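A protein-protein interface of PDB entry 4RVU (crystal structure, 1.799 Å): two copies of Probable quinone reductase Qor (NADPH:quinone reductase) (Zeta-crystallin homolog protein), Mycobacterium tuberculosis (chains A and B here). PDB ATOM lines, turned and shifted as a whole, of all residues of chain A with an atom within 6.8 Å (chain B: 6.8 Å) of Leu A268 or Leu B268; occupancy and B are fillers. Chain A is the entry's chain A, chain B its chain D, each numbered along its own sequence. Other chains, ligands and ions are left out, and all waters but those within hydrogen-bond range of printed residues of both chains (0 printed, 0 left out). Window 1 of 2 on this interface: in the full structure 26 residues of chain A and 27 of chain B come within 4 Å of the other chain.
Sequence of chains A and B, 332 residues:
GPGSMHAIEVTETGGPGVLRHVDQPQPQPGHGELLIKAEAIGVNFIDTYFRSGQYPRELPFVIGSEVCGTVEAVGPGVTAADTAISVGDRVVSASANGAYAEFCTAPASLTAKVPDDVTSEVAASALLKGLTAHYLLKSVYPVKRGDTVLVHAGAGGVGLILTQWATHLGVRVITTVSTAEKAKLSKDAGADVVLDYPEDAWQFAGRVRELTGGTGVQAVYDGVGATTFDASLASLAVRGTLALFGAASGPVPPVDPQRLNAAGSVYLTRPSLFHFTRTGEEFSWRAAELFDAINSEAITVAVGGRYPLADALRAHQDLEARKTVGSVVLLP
O of Leu B268 sits at hydrogen-bond distance from N of Leu A268 (2.7 Å). The backbone carbonyl oxygen of Val B266 sits at hydrogen-bond distance from the side-chain hydroxyl of Thr A269, 2.9 Å away. The backbone carbonyl oxygen (O) of Val A266 is in hydrogen-bond range of the side-chain hydroxyl (OG1) of Thr B269, 2.7 Å away. O of Val B255 is in hydrogen-bond range of N of Val A255 (2.9 Å).
The backbone NH (N) of Leu A242 is in hydrogen-bond range of the backbone carbonyl oxygen (O) of Tyr A267 (2.8 Å). The backbone NH (N) of Leu B244 sits at hydrogen-bond distance from the backbone carbonyl oxygen (O) of Thr B269 (3.0 Å). The backbone carbonyl oxygen (O) of Thr A269 is in hydrogen-bond range of the backbone NH (N) of Leu A244 (3.0 Å). The backbone carbonyl oxygen of Tyr B267 is in hydrogen-bond range of the backbone NH of Leu B242, 2.9 Å away. The backbone carbonyl oxygen (O) of Leu A242 lies within hydrogen-bond range of the backbone NH (N) of Thr A269. N of Tyr A267 lies within hydrogen-bond range of O of Gly A240.
Among the printed residues, pairs that only touch across the chains: Leu A244 with Pro B257, Val A255 with Pro B257, Pro A257 with Leu B244, Pro A257 with Val B255, Pro A257 with Arg B270, Leu A260 with Leu B268, Val A266 with Arg B270, Tyr A267 with Leu B268, Tyr A267 with Thr B269, Leu A268 with Leu B260, Leu A268 with Tyr B267, Thr A269 with Tyr B267, Arg A270 with Pro B257 and Arg A270 with Leu B260.
Thr A241 touches none of the printed residues of chain B. Printed residues of chain B within 4 Å of Val A255: Val B255 and Pro B257. Printed residues of chain B within 4 Å of Pro A257: Leu B244, Val B255 and Arg B270. Of chain B, only Leu B260 (3.7 Å), Tyr B267 (3.5 Å) and Leu B268 (2.7 Å) come within 4 Å of Leu A268. Of the printed residues of chain B, Thr A269 touches Val B266 and Tyr B267. Of the printed residues of chain B, Arg A270 touches Pro B257 (3.3 Å) and Leu B260 (3.999 Å). Gly B240 touches none of the printed residues of chain A. Of the printed residues of chain A, Leu B244 touches Pro A257 (3.6 Å). Leu B268 touches just these residues of chain A: Leu A260, Tyr A267 and Leu A268. The nearest residue of chain B that does not touch Leu A268 is Val B266 (4.03 Å). The nearest printed residue of chain B that does not touch Arg A270 is Val B266 (4.1 Å).
Of the 16 printed residues of chain A, 9 touch a printed residue of chain B. Of the 16 printed residues of chain B, 9 touch a printed residue of chain A. Hydrophobic or aromatic side chains of chain B that line the printed part of chain A: Leu B244, Val B255, Pro B257, Leu B260, Tyr B267 and Leu B268. Among the printed residues, 18 pairs touch across the chains.
Leu A260 touches Leu B268, and with the chains exchanged Leu A268 touches Leu B260. Val A266 touches Thr B269, and with the chains exchanged Thr A269 touches Val B266. Tyr A267 touches Thr B269, and with the chains exchanged Thr A269 touches Tyr B267. Leu A268 touches its own counterpart, Leu B268. Of the 18 pairs that touch across the chains among the printed residues, 16 have their exchanged pair printed and touching as well.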
ATOM      1  N   PHE A 229       7.839 -28.009 -14.190  1.00  0.00           N
ATOM      2  CA  PHE A 229       6.891 -27.443 -15.158  1.00  0.00           C
ATOM      3  C   PHE A 229       5.437 -27.868 -14.919  1.00  0.00           C
ATOM      4  O   PHE A 229       4.536 -27.017 -14.864  1.00  0.00           O
ATOM      5  CB  PHE A 229       7.290 -27.750 -16.606  1.00  0.00           C
ATOM      6  CG  PHE A 229       6.412 -27.067 -17.613  1.00  0.00           C
ATOM      7  CD1 PHE A 229       5.269 -27.695 -18.091  1.00  0.00           C
ATOM      8  CD2 PHE A 229       6.701 -25.780 -18.048  1.00  0.00           C
ATOM      9  CE1 PHE A 229       4.441 -27.070 -19.002  1.00  0.00           C
ATOM     10  CE2 PHE A 229       5.871 -25.141 -18.968  1.00  0.00           C
ATOM     11  CZ  PHE A 229       4.736 -25.797 -19.443  1.00  0.00           C
ATOM     12  N   LEU A 233       2.460 -25.241 -14.041  1.00  0.00           N
ATOM     13  CA  LEU A 233       1.256 -25.102 -14.863  1.00  0.00           C
ATOM     14  C   LEU A 233      -0.014 -25.336 -14.031  1.00  0.00           C
ATOM     15  O   LEU A 233      -1.005 -24.608 -14.162  1.00  0.00           O
ATOM     16  CB  LEU A 233       1.319 -26.054 -16.063  1.00  0.00           C
ATOM     17  CG  LEU A 233       0.115 -26.011 -17.013  1.00  0.00           C
ATOM     18  CD1 LEU A 233      -0.009 -24.625 -17.602  1.00  0.00           C
ATOM     19  CD2 LEU A 233       0.236 -27.039 -18.119  1.00  0.00           C
ATOM     20  N   GLY A 240      -3.589 -16.814 -15.861  1.00  0.00           N
ATOM     21  CA  GLY A 240      -2.294 -16.477 -15.291  1.00  0.00           C
ATOM     22  C   GLY A 240      -1.176 -16.704 -16.291  1.00  0.00           C
ATOM     23  O   GLY A 240      -1.397 -17.252 -17.365  1.00  0.00           O
ATOM     24  N   THR A 241       0.039 -16.288 -15.944  1.00  0.00           N
ATOM     25  CA  THR A 241       1.160 -16.387 -16.885  1.00  0.00           C
ATOM     26  C   THR A 241       2.237 -17.318 -16.357  1.00  0.00           C
ATOM     27  O   THR A 241       2.751 -17.112 -15.259  1.00  0.00           O
ATOM     28  CB  THR A 241       1.796 -15.007 -17.143  1.00  0.00           C
ATOM     29  OG1 THR A 241       0.868 -14.166 -17.842  1.00  0.00           O
ATOM     30  CG2 THR A 241       3.076 -15.148 -17.971  1.00  0.00           C
ATOM     31  N   LEU A 242       2.567 -18.344 -17.132  1.00  0.00           N
ATOM     32  CA  LEU A 242       3.705 -19.196 -16.821  1.00  0.00           C
ATOM     33  C   LEU A 242       4.903 -18.665 -17.598  1.00  0.00           C
ATOM     34  O   LEU A 242       4.974 -18.798 -18.821  1.00  0.00           O
ATOM     35  CB  LEU A 242       3.427 -20.649 -17.220  1.00  0.00           C
ATOM     36  CG  LEU A 242       4.110 -21.738 -16.387  1.00  0.00           C
ATOM     37  CD1 LEU A 242       3.709 -23.129 -16.847  1.00  0.00           C
ATOM     38  CD2 LEU A 242       5.631 -21.606 -16.406  1.00  0.00           C
ATOM     39  N   ALA A 243       5.841 -18.043 -16.892  1.00  0.00           N
ATOM     40  CA  ALA A 243       7.076 -17.608 -17.527  1.00  0.00           C
ATOM     41  C   ALA A 243       8.127 -18.673 -17.276  1.00  0.00           C
ATOM     42  O   ALA A 243       8.732 -18.733 -16.194  1.00  0.00           O
ATOM     43  CB  ALA A 243       7.520 -16.260 -16.994  1.00  0.00           C
ATOM     44  N   LEU A 244       8.321 -19.532 -18.272  1.00  0.00           N
ATOM     45  CA  LEU A 244       9.372 -20.551 -18.226  1.00  0.00           C
ATOM     46  C   LEU A 244      10.646 -19.924 -18.775  1.00  0.00           C
ATOM     47  O   LEU A 244      10.811 -19.813 -19.992  1.00  0.00           O
ATOM     48  CB  LEU A 244       8.963 -21.757 -19.079  1.00  0.00           C
ATOM     49  CG  LEU A 244      10.002 -22.866 -19.271  1.00  0.00           C
ATOM     50  CD1 LEU A 244      10.346 -23.520 -17.933  1.00  0.00           C
ATOM     51  CD2 LEU A 244       9.487 -23.898 -20.250  1.00  0.00           C
ATOM     52  N   VAL A 255       4.782 -29.357 -24.997  1.00  0.00           N
ATOM     53  CA  VAL A 255       3.557 -29.109 -24.238  1.00  0.00           C
ATOM     54  C   VAL A 255       2.331 -29.082 -25.144  1.00  0.00           C
ATOM     55  O   VAL A 255       2.226 -28.220 -26.018  1.00  0.00           O
ATOM     56  CB  VAL A 255       3.643 -27.756 -23.492  1.00  0.00           C
ATOM     57  CG1 VAL A 255       2.356 -27.467 -22.739  1.00  0.00           C
ATOM     58  CG2 VAL A 255       4.858 -27.734 -22.532  1.00  0.00           C
ATOM     59  N   ASP A 256       1.406 -30.021 -24.947  1.00  0.00           N
ATOM     60  CA  ASP A 256       0.109 -29.968 -25.632  1.00  0.00           C
ATOM     61  C   ASP A 256      -0.556 -28.638 -25.291  1.00  0.00           C
ATOM     62  O   ASP A 256      -0.833 -28.382 -24.122  1.00  0.00           O
ATOM     63  CB  ASP A 256      -0.777 -31.115 -25.138  1.00  0.00           C
ATOM     64  CG  ASP A 256      -2.140 -31.171 -25.832  1.00  0.00           C
ATOM     65  OD1 ASP A 256      -2.585 -30.173 -26.428  1.00  0.00           O
ATOM     66  OD2 ASP A 256      -2.778 -32.241 -25.761  1.00  0.00           O
ATOM     67  N   PRO A 257      -0.811 -27.783 -26.305  1.00  0.00           N
ATOM     68  CA  PRO A 257      -1.413 -26.476 -26.017  1.00  0.00           C
ATOM     69  C   PRO A 257      -2.736 -26.578 -25.278  1.00  0.00           C
ATOM     70  O   PRO A 257      -3.080 -25.659 -24.534  1.00  0.00           O
ATOM     71  CB  PRO A 257      -1.625 -25.879 -27.412  1.00  0.00           C
ATOM     72  CG  PRO A 257      -0.544 -26.497 -28.237  1.00  0.00           C
ATOM     73  CD  PRO A 257      -0.450 -27.913 -27.731  1.00  0.00           C
ATOM     74  N   LEU A 260      -2.905 -25.781 -21.684  1.00  0.00           N
ATOM     75  CA  LEU A 260      -3.000 -24.380 -21.263  1.00  0.00           C
ATOM     76  C   LEU A 260      -4.459 -23.972 -21.088  1.00  0.00           C
ATOM     77  O   LEU A 260      -4.789 -23.104 -20.279  1.00  0.00           O
ATOM     78  CB  LEU A 260      -2.305 -23.459 -22.273  1.00  0.00           C
ATOM     79  CG  LEU A 260      -0.864 -23.779 -22.664  1.00  0.00           C
ATOM     80  CD1 LEU A 260      -0.327 -22.745 -23.659  1.00  0.00           C
ATOM     81  CD2 LEU A 260       0.046 -23.841 -21.427  1.00  0.00           C
ATOM     82  N   VAL A 266      -4.474 -20.147 -19.699  1.00  0.00           N
ATOM     83  CA  VAL A 266      -3.305 -19.434 -19.216  1.00  0.00           C
ATOM     84  C   VAL A 266      -2.390 -19.090 -20.375  1.00  0.00           C
ATOM     85  O   VAL A 266      -2.603 -19.539 -21.504  1.00  0.00           O
ATOM     86  CB  VAL A 266      -2.542 -20.269 -18.188  1.00  0.00           C
ATOM     87  CG1 VAL A 266      -3.493 -20.723 -17.087  1.00  0.00           C
ATOM     88  CG2 VAL A 266      -1.887 -21.464 -18.856  1.00  0.00           C
ATOM     89  N   TYR A 267      -1.377 -18.281 -20.087  1.00  0.00           N
ATOM     90  CA  TYR A 267      -0.363 -17.945 -21.073  1.00  0.00           C
ATOM     91  C   TYR A 267       0.893 -18.704 -20.732  1.00  0.00           C
ATOM     92  O   TYR A 267       1.255 -18.807 -19.547  1.00  0.00           O
ATOM     93  CB  TYR A 267       0.006 -16.470 -20.980  1.00  0.00           C
ATOM     94  CG  TYR A 267      -1.098 -15.494 -21.268  1.00  0.00           C
ATOM     95  CD1 TYR A 267      -1.995 -15.125 -20.278  1.00  0.00           C
ATOM     96  CD2 TYR A 267      -1.224 -14.908 -22.524  1.00  0.00           C
ATOM     97  CE1 TYR A 267      -2.998 -14.216 -20.530  1.00  0.00           C
ATOM     98  CE2 TYR A 267      -2.234 -13.998 -22.788  1.00  0.00           C
ATOM     99  CZ  TYR A 267      -3.106 -13.651 -21.779  1.00  0.00           C
ATOM    100  OH  TYR A 267      -4.104 -12.734 -22.021  1.00  0.00           O
ATOM    101  N   LEU A 268       1.569 -19.206 -21.762  1.00  0.00           N
ATOM    102  CA  LEU A 268       2.909 -19.770 -21.608  1.00  0.00           C
ATOM    103  C   LEU A 268       3.887 -18.916 -22.407  1.00  0.00           C
ATOM    104  O   LEU A 268       3.652 -18.598 -23.575  1.00  0.00           O
ATOM    105  CB  LEU A 268       2.949 -21.232 -22.083  1.00  0.00           C
ATOM    106  CG  LEU A 268       4.305 -21.942 -22.084  1.00  0.00           C
ATOM    107  CD1 LEU A 268       4.857 -22.112 -20.653  1.00  0.00           C
ATOM    108  CD2 LEU A 268       4.217 -23.281 -22.790  1.00  0.00           C
ATOM    109  N   THR A 269       4.993 -18.519 -21.787  1.00  0.00           N
ATOM    110  CA  THR A 269       5.997 -17.802 -22.552  1.00  0.00           C
ATOM    111  C   THR A 269       7.371 -18.303 -22.155  1.00  0.00           C
ATOM    112  O   THR A 269       7.586 -18.662 -21.000  1.00  0.00           O
ATOM    113  CB  THR A 269       5.882 -16.279 -22.346  1.00  0.00           C
ATOM    114  OG1 THR A 269       6.891 -15.616 -23.126  1.00  0.00           O
ATOM    115  CG2 THR A 269       6.080 -15.928 -20.866  1.00  0.00           C
ATOM    116  N   ARG A 270       8.295 -18.342 -23.112  1.00  0.00           N
ATOM    117  CA  ARG A 270       9.668 -18.774 -22.827  1.00  0.00           C
ATOM    118  C   ARG A 270      10.610 -17.667 -23.277  1.00  0.00           C
ATOM    119  O   ARG A 270      11.110 -17.693 -24.404  1.00  0.00           O
ATOM    120  CB  ARG A 270      10.003 -20.077 -23.564  1.00  0.00           C
ATOM    121  CG  ARG A 270      11.121 -20.932 -22.904  1.00  0.00           C
ATOM    122  CD  ARG A 270      12.450 -20.176 -22.750  1.00  0.00           C
ATOM    123  NE  ARG A 270      13.491 -20.961 -22.085  1.00  0.00           N
ATOM    124  CZ  ARG A 270      14.695 -20.492 -21.763  1.00  0.00           C
ATOM    125  NH1 ARG A 270      15.022 -19.234 -22.022  1.00  0.00           N
ATOM    126  NH2 ARG A 270      15.580 -21.281 -21.168  1.00  0.00           N
ATOM    127  N   PHE B 229      -0.439 -23.670 -37.464  1.00  0.00           N
ATOM    128  CA  PHE B 229       0.236 -23.289 -36.226  1.00  0.00           C
ATOM    129  C   PHE B 229       1.678 -22.844 -36.442  1.00  0.00           C
ATOM    130  O   PHE B 229       2.090 -21.804 -35.923  1.00  0.00           O
ATOM    131  CB  PHE B 229       0.172 -24.379 -35.155  1.00  0.00           C
ATOM    132  CG  PHE B 229       0.800 -23.957 -33.853  1.00  0.00           C
ATOM    133  CD1 PHE B 229       2.142 -24.212 -33.602  1.00  0.00           C
ATOM    134  CD2 PHE B 229       0.059 -23.269 -32.900  1.00  0.00           C
ATOM    135  CE1 PHE B 229       2.743 -23.794 -32.401  1.00  0.00           C
ATOM    136  CE2 PHE B 229       0.636 -22.853 -31.701  1.00  0.00           C
ATOM    137  CZ  PHE B 229       1.989 -23.115 -31.454  1.00  0.00           C
ATOM    138  N   LEU B 233       3.168 -19.067 -35.600  1.00  0.00           N
ATOM    139  CA  LEU B 233       4.275 -18.870 -34.662  1.00  0.00           C
ATOM    140  C   LEU B 233       5.413 -18.089 -35.321  1.00  0.00           C
ATOM    141  O   LEU B 233       6.009 -17.208 -34.707  1.00  0.00           O
ATOM    142  CB  LEU B 233       4.762 -20.231 -34.168  1.00  0.00           C
ATOM    143  CG  LEU B 233       5.872 -20.230 -33.121  1.00  0.00           C
ATOM    144  CD1 LEU B 233       5.467 -19.316 -31.992  1.00  0.00           C
ATOM    145  CD2 LEU B 233       6.117 -21.638 -32.610  1.00  0.00           C
ATOM    146  N   GLY B 240       5.121 -10.955 -29.225  1.00  0.00           N
ATOM    147  CA  GLY B 240       3.736 -11.022 -29.680  1.00  0.00           C
ATOM    148  C   GLY B 240       2.953 -12.155 -29.036  1.00  0.00           C
ATOM    149  O   GLY B 240       3.516 -12.990 -28.318  1.00  0.00           O
ATOM    150  N   THR B 241       1.647 -12.194 -29.289  1.00  0.00           N
ATOM    151  CA  THR B 241       0.789 -13.214 -28.679  1.00  0.00           C
ATOM    152  C   THR B 241       0.142 -14.106 -29.727  1.00  0.00           C
ATOM    153  O   THR B 241      -0.516 -13.629 -30.648  1.00  0.00           O
ATOM    154  CB  THR B 241      -0.304 -12.598 -27.800  1.00  0.00           C
ATOM    155  OG1 THR B 241       0.301 -11.884 -26.717  1.00  0.00           O
ATOM    156  CG2 THR B 241      -1.223 -13.703 -27.226  1.00  0.00           C
ATOM    157  N   LEU B 242       0.360 -15.407 -29.589  1.00  0.00           N
ATOM    158  CA  LEU B 242      -0.306 -16.396 -30.429  1.00  0.00           C
ATOM    159  C   LEU B 242      -1.511 -16.893 -29.633  1.00  0.00           C
ATOM    160  O   LEU B 242      -1.363 -17.627 -28.642  1.00  0.00           O
ATOM    161  CB  LEU B 242       0.662 -17.537 -30.772  1.00  0.00           C
ATOM    162  CG  LEU B 242       0.272 -18.837 -31.498  1.00  0.00           C
ATOM    163  CD1 LEU B 242      -1.119 -18.843 -32.154  1.00  0.00           C
ATOM    164  CD2 LEU B 242       1.341 -19.268 -32.493  1.00  0.00           C
ATOM    165  N   ALA B 243      -2.698 -16.445 -30.034  1.00  0.00           N
ATOM    166  CA  ALA B 243      -3.938 -16.927 -29.428  1.00  0.00           C
ATOM    167  C   ALA B 243      -4.470 -18.086 -30.251  1.00  0.00           C
ATOM    168  O   ALA B 243      -5.157 -17.888 -31.270  1.00  0.00           O
ATOM    169  CB  ALA B 243      -4.963 -15.814 -29.334  1.00  0.00           C
ATOM    170  N   LEU B 244      -4.129 -19.297 -29.817  1.00  0.00           N
ATOM    171  CA  LEU B 244      -4.618 -20.522 -30.437  1.00  0.00           C
ATOM    172  C   LEU B 244      -5.947 -20.876 -29.797  1.00  0.00           C
ATOM    173  O   LEU B 244      -5.983 -21.466 -28.719  1.00  0.00           O
ATOM    174  CB  LEU B 244      -3.604 -21.658 -30.242  1.00  0.00           C
ATOM    175  CG  LEU B 244      -4.016 -23.045 -30.758  1.00  0.00           C
ATOM    176  CD1 LEU B 244      -4.095 -23.059 -32.277  1.00  0.00           C
ATOM    177  CD2 LEU B 244      -3.058 -24.115 -30.259  1.00  0.00           C
ATOM    178  N   VAL B 255       4.005 -28.623 -28.246  1.00  0.00           N
ATOM    179  CA  VAL B 255       4.902 -27.537 -28.655  1.00  0.00           C
ATOM    180  C   VAL B 255       6.119 -27.435 -27.731  1.00  0.00           C
ATOM    181  O   VAL B 255       5.965 -27.234 -26.528  1.00  0.00           O
ATOM    182  CB  VAL B 255       4.152 -26.175 -28.674  1.00  0.00           C
ATOM    183  CG1 VAL B 255       5.104 -25.028 -28.988  1.00  0.00           C
ATOM    184  CG2 VAL B 255       3.019 -26.214 -29.715  1.00  0.00           C
ATOM    185  N   ASP B 256       7.316 -27.597 -28.294  1.00  0.00           N
ATOM    186  CA  ASP B 256       8.562 -27.423 -27.537  1.00  0.00           C
ATOM    187  C   ASP B 256       8.608 -25.969 -27.101  1.00  0.00           C
ATOM    188  O   ASP B 256       8.624 -25.089 -27.946  1.00  0.00           O
ATOM    189  CB  ASP B 256       9.767 -27.739 -28.430  1.00  0.00           C
ATOM    190  CG  ASP B 256      11.112 -27.549 -27.718  1.00  0.00           C
ATOM    191  OD1 ASP B 256      11.159 -27.013 -26.589  1.00  0.00           O
ATOM    192  OD2 ASP B 256      12.144 -27.935 -28.306  1.00  0.00           O
ATOM    193  N   PRO B 257       8.615 -25.715 -25.783  1.00  0.00           N
ATOM    194  CA  PRO B 257       8.591 -24.324 -25.311  1.00  0.00           C
ATOM    195  C   PRO B 257       9.739 -23.475 -25.855  1.00  0.00           C
ATOM    196  O   PRO B 257       9.594 -22.253 -25.969  1.00  0.00           O
ATOM    197  CB  PRO B 257       8.721 -24.473 -23.796  1.00  0.00           C
ATOM    198  CG  PRO B 257       8.112 -25.825 -23.503  1.00  0.00           C
ATOM    199  CD  PRO B 257       8.554 -26.678 -24.664  1.00  0.00           C
ATOM    200  N   LEU B 260       9.052 -21.031 -28.577  1.00  0.00           N
ATOM    201  CA  LEU B 260       8.493 -19.726 -28.207  1.00  0.00           C
ATOM    202  C   LEU B 260       9.610 -18.717 -27.967  1.00  0.00           C
ATOM    203  O   LEU B 260       9.439 -17.516 -28.174  1.00  0.00           O
ATOM    204  CB  LEU B 260       7.606 -19.835 -26.958  1.00  0.00           C
ATOM    205  CG  LEU B 260       6.519 -20.910 -26.952  1.00  0.00           C
ATOM    206  CD1 LEU B 260       5.728 -20.880 -25.647  1.00  0.00           C
ATOM    207  CD2 LEU B 260       5.582 -20.746 -28.150  1.00  0.00           C
ATOM    208  N   VAL B 266       7.804 -15.052 -27.495  1.00  0.00           N
ATOM    209  CA  VAL B 266       6.385 -14.816 -27.694  1.00  0.00           C
ATOM    210  C   VAL B 266       5.562 -15.506 -26.611  1.00  0.00           C
ATOM    211  O   VAL B 266       6.075 -16.340 -25.864  1.00  0.00           O
ATOM    212  CB  VAL B 266       5.924 -15.290 -29.077  1.00  0.00           C
ATOM    213  CG1 VAL B 266       6.785 -14.666 -30.171  1.00  0.00           C
ATOM    214  CG2 VAL B 266       5.977 -16.812 -29.179  1.00  0.00           C
ATOM    215  N   TYR B 267       4.282 -15.145 -26.537  1.00  0.00           N
ATOM    216  CA  TYR B 267       3.362 -15.795 -25.621  1.00  0.00           C
ATOM    217  C   TYR B 267       2.522 -16.762 -26.424  1.00  0.00           C
ATOM    218  O   TYR B 267       2.117 -16.442 -27.547  1.00  0.00           O
ATOM    219  CB  TYR B 267       2.402 -14.775 -25.027  1.00  0.00           C
ATOM    220  CG  TYR B 267       3.008 -13.697 -24.167  1.00  0.00           C
ATOM    221  CD1 TYR B 267       3.014 -13.815 -22.784  1.00  0.00           C
ATOM    222  CD2 TYR B 267       3.528 -12.536 -24.736  1.00  0.00           C
ATOM    223  CE1 TYR B 267       3.544 -12.813 -21.985  1.00  0.00           C
ATOM    224  CE2 TYR B 267       4.058 -11.533 -23.949  1.00  0.00           C
ATOM    225  CZ  TYR B 267       4.061 -11.678 -22.575  1.00  0.00           C
ATOM    226  OH  TYR B 267       4.579 -10.672 -21.788  1.00  0.00           O
ATOM    227  N   LEU B 268       2.238 -17.929 -25.851  1.00  0.00           N
ATOM    228  CA  LEU B 268       1.267 -18.845 -26.438  1.00  0.00           C
ATOM    229  C   LEU B 268       0.143 -19.026 -25.436  1.00  0.00           C
ATOM    230  O   LEU B 268       0.389 -19.224 -24.239  1.00  0.00           O
ATOM    231  CB  LEU B 268       1.909 -20.203 -26.737  1.00  0.00           C
ATOM    232  CG  LEU B 268       0.937 -21.328 -27.096  1.00  0.00           C
ATOM    233  CD1 LEU B 268       0.266 -21.023 -28.449  1.00  0.00           C
ATOM    234  CD2 LEU B 268       1.696 -22.643 -27.163  1.00  0.00           C
ATOM    235  N   THR B 269      -1.100 -18.937 -25.901  1.00  0.00           N
ATOM    236  CA  THR B 269      -2.222 -19.148 -24.995  1.00  0.00           C
ATOM    237  C   THR B 269      -3.319 -19.905 -25.723  1.00  0.00           C
ATOM    238  O   THR B 269      -3.527 -19.706 -26.925  1.00  0.00           O
ATOM    239  CB  THR B 269      -2.750 -17.814 -24.385  1.00  0.00           C
ATOM    240  OG1 THR B 269      -3.834 -18.082 -23.480  1.00  0.00           O
ATOM    241  CG2 THR B 269      -3.226 -16.873 -25.475  1.00  0.00           C
ATOM    242  N   ARG B 270      -3.990 -20.807 -25.007  1.00  0.00           N
ATOM    243  CA  ARG B 270      -5.111 -21.561 -25.589  1.00  0.00           C
ATOM    244  C   ARG B 270      -6.372 -21.278 -24.781  1.00  0.00           C
ATOM    245  O   ARG B 270      -6.681 -22.000 -23.838  1.00  0.00           O
ATOM    246  CB  ARG B 270      -4.817 -23.066 -25.594  1.00  0.00           C
ATOM    247  CG  ARG B 270      -5.447 -23.828 -26.762  1.00  0.00           C
ATOM    248  CD  ARG B 270      -6.960 -23.692 -26.796  1.00  0.00           C
ATOM    249  NE  ARG B 270      -7.570 -24.424 -27.904  1.00  0.00           N
ATOM    250  CZ  ARG B 270      -8.880 -24.483 -28.123  1.00  0.00           C
ATOM    251  NH1 ARG B 270      -9.721 -23.847 -27.323  1.00  0.00           N
ATOM    252  NH2 ARG B 270      -9.353 -25.183 -29.146  1.00  0.00           N
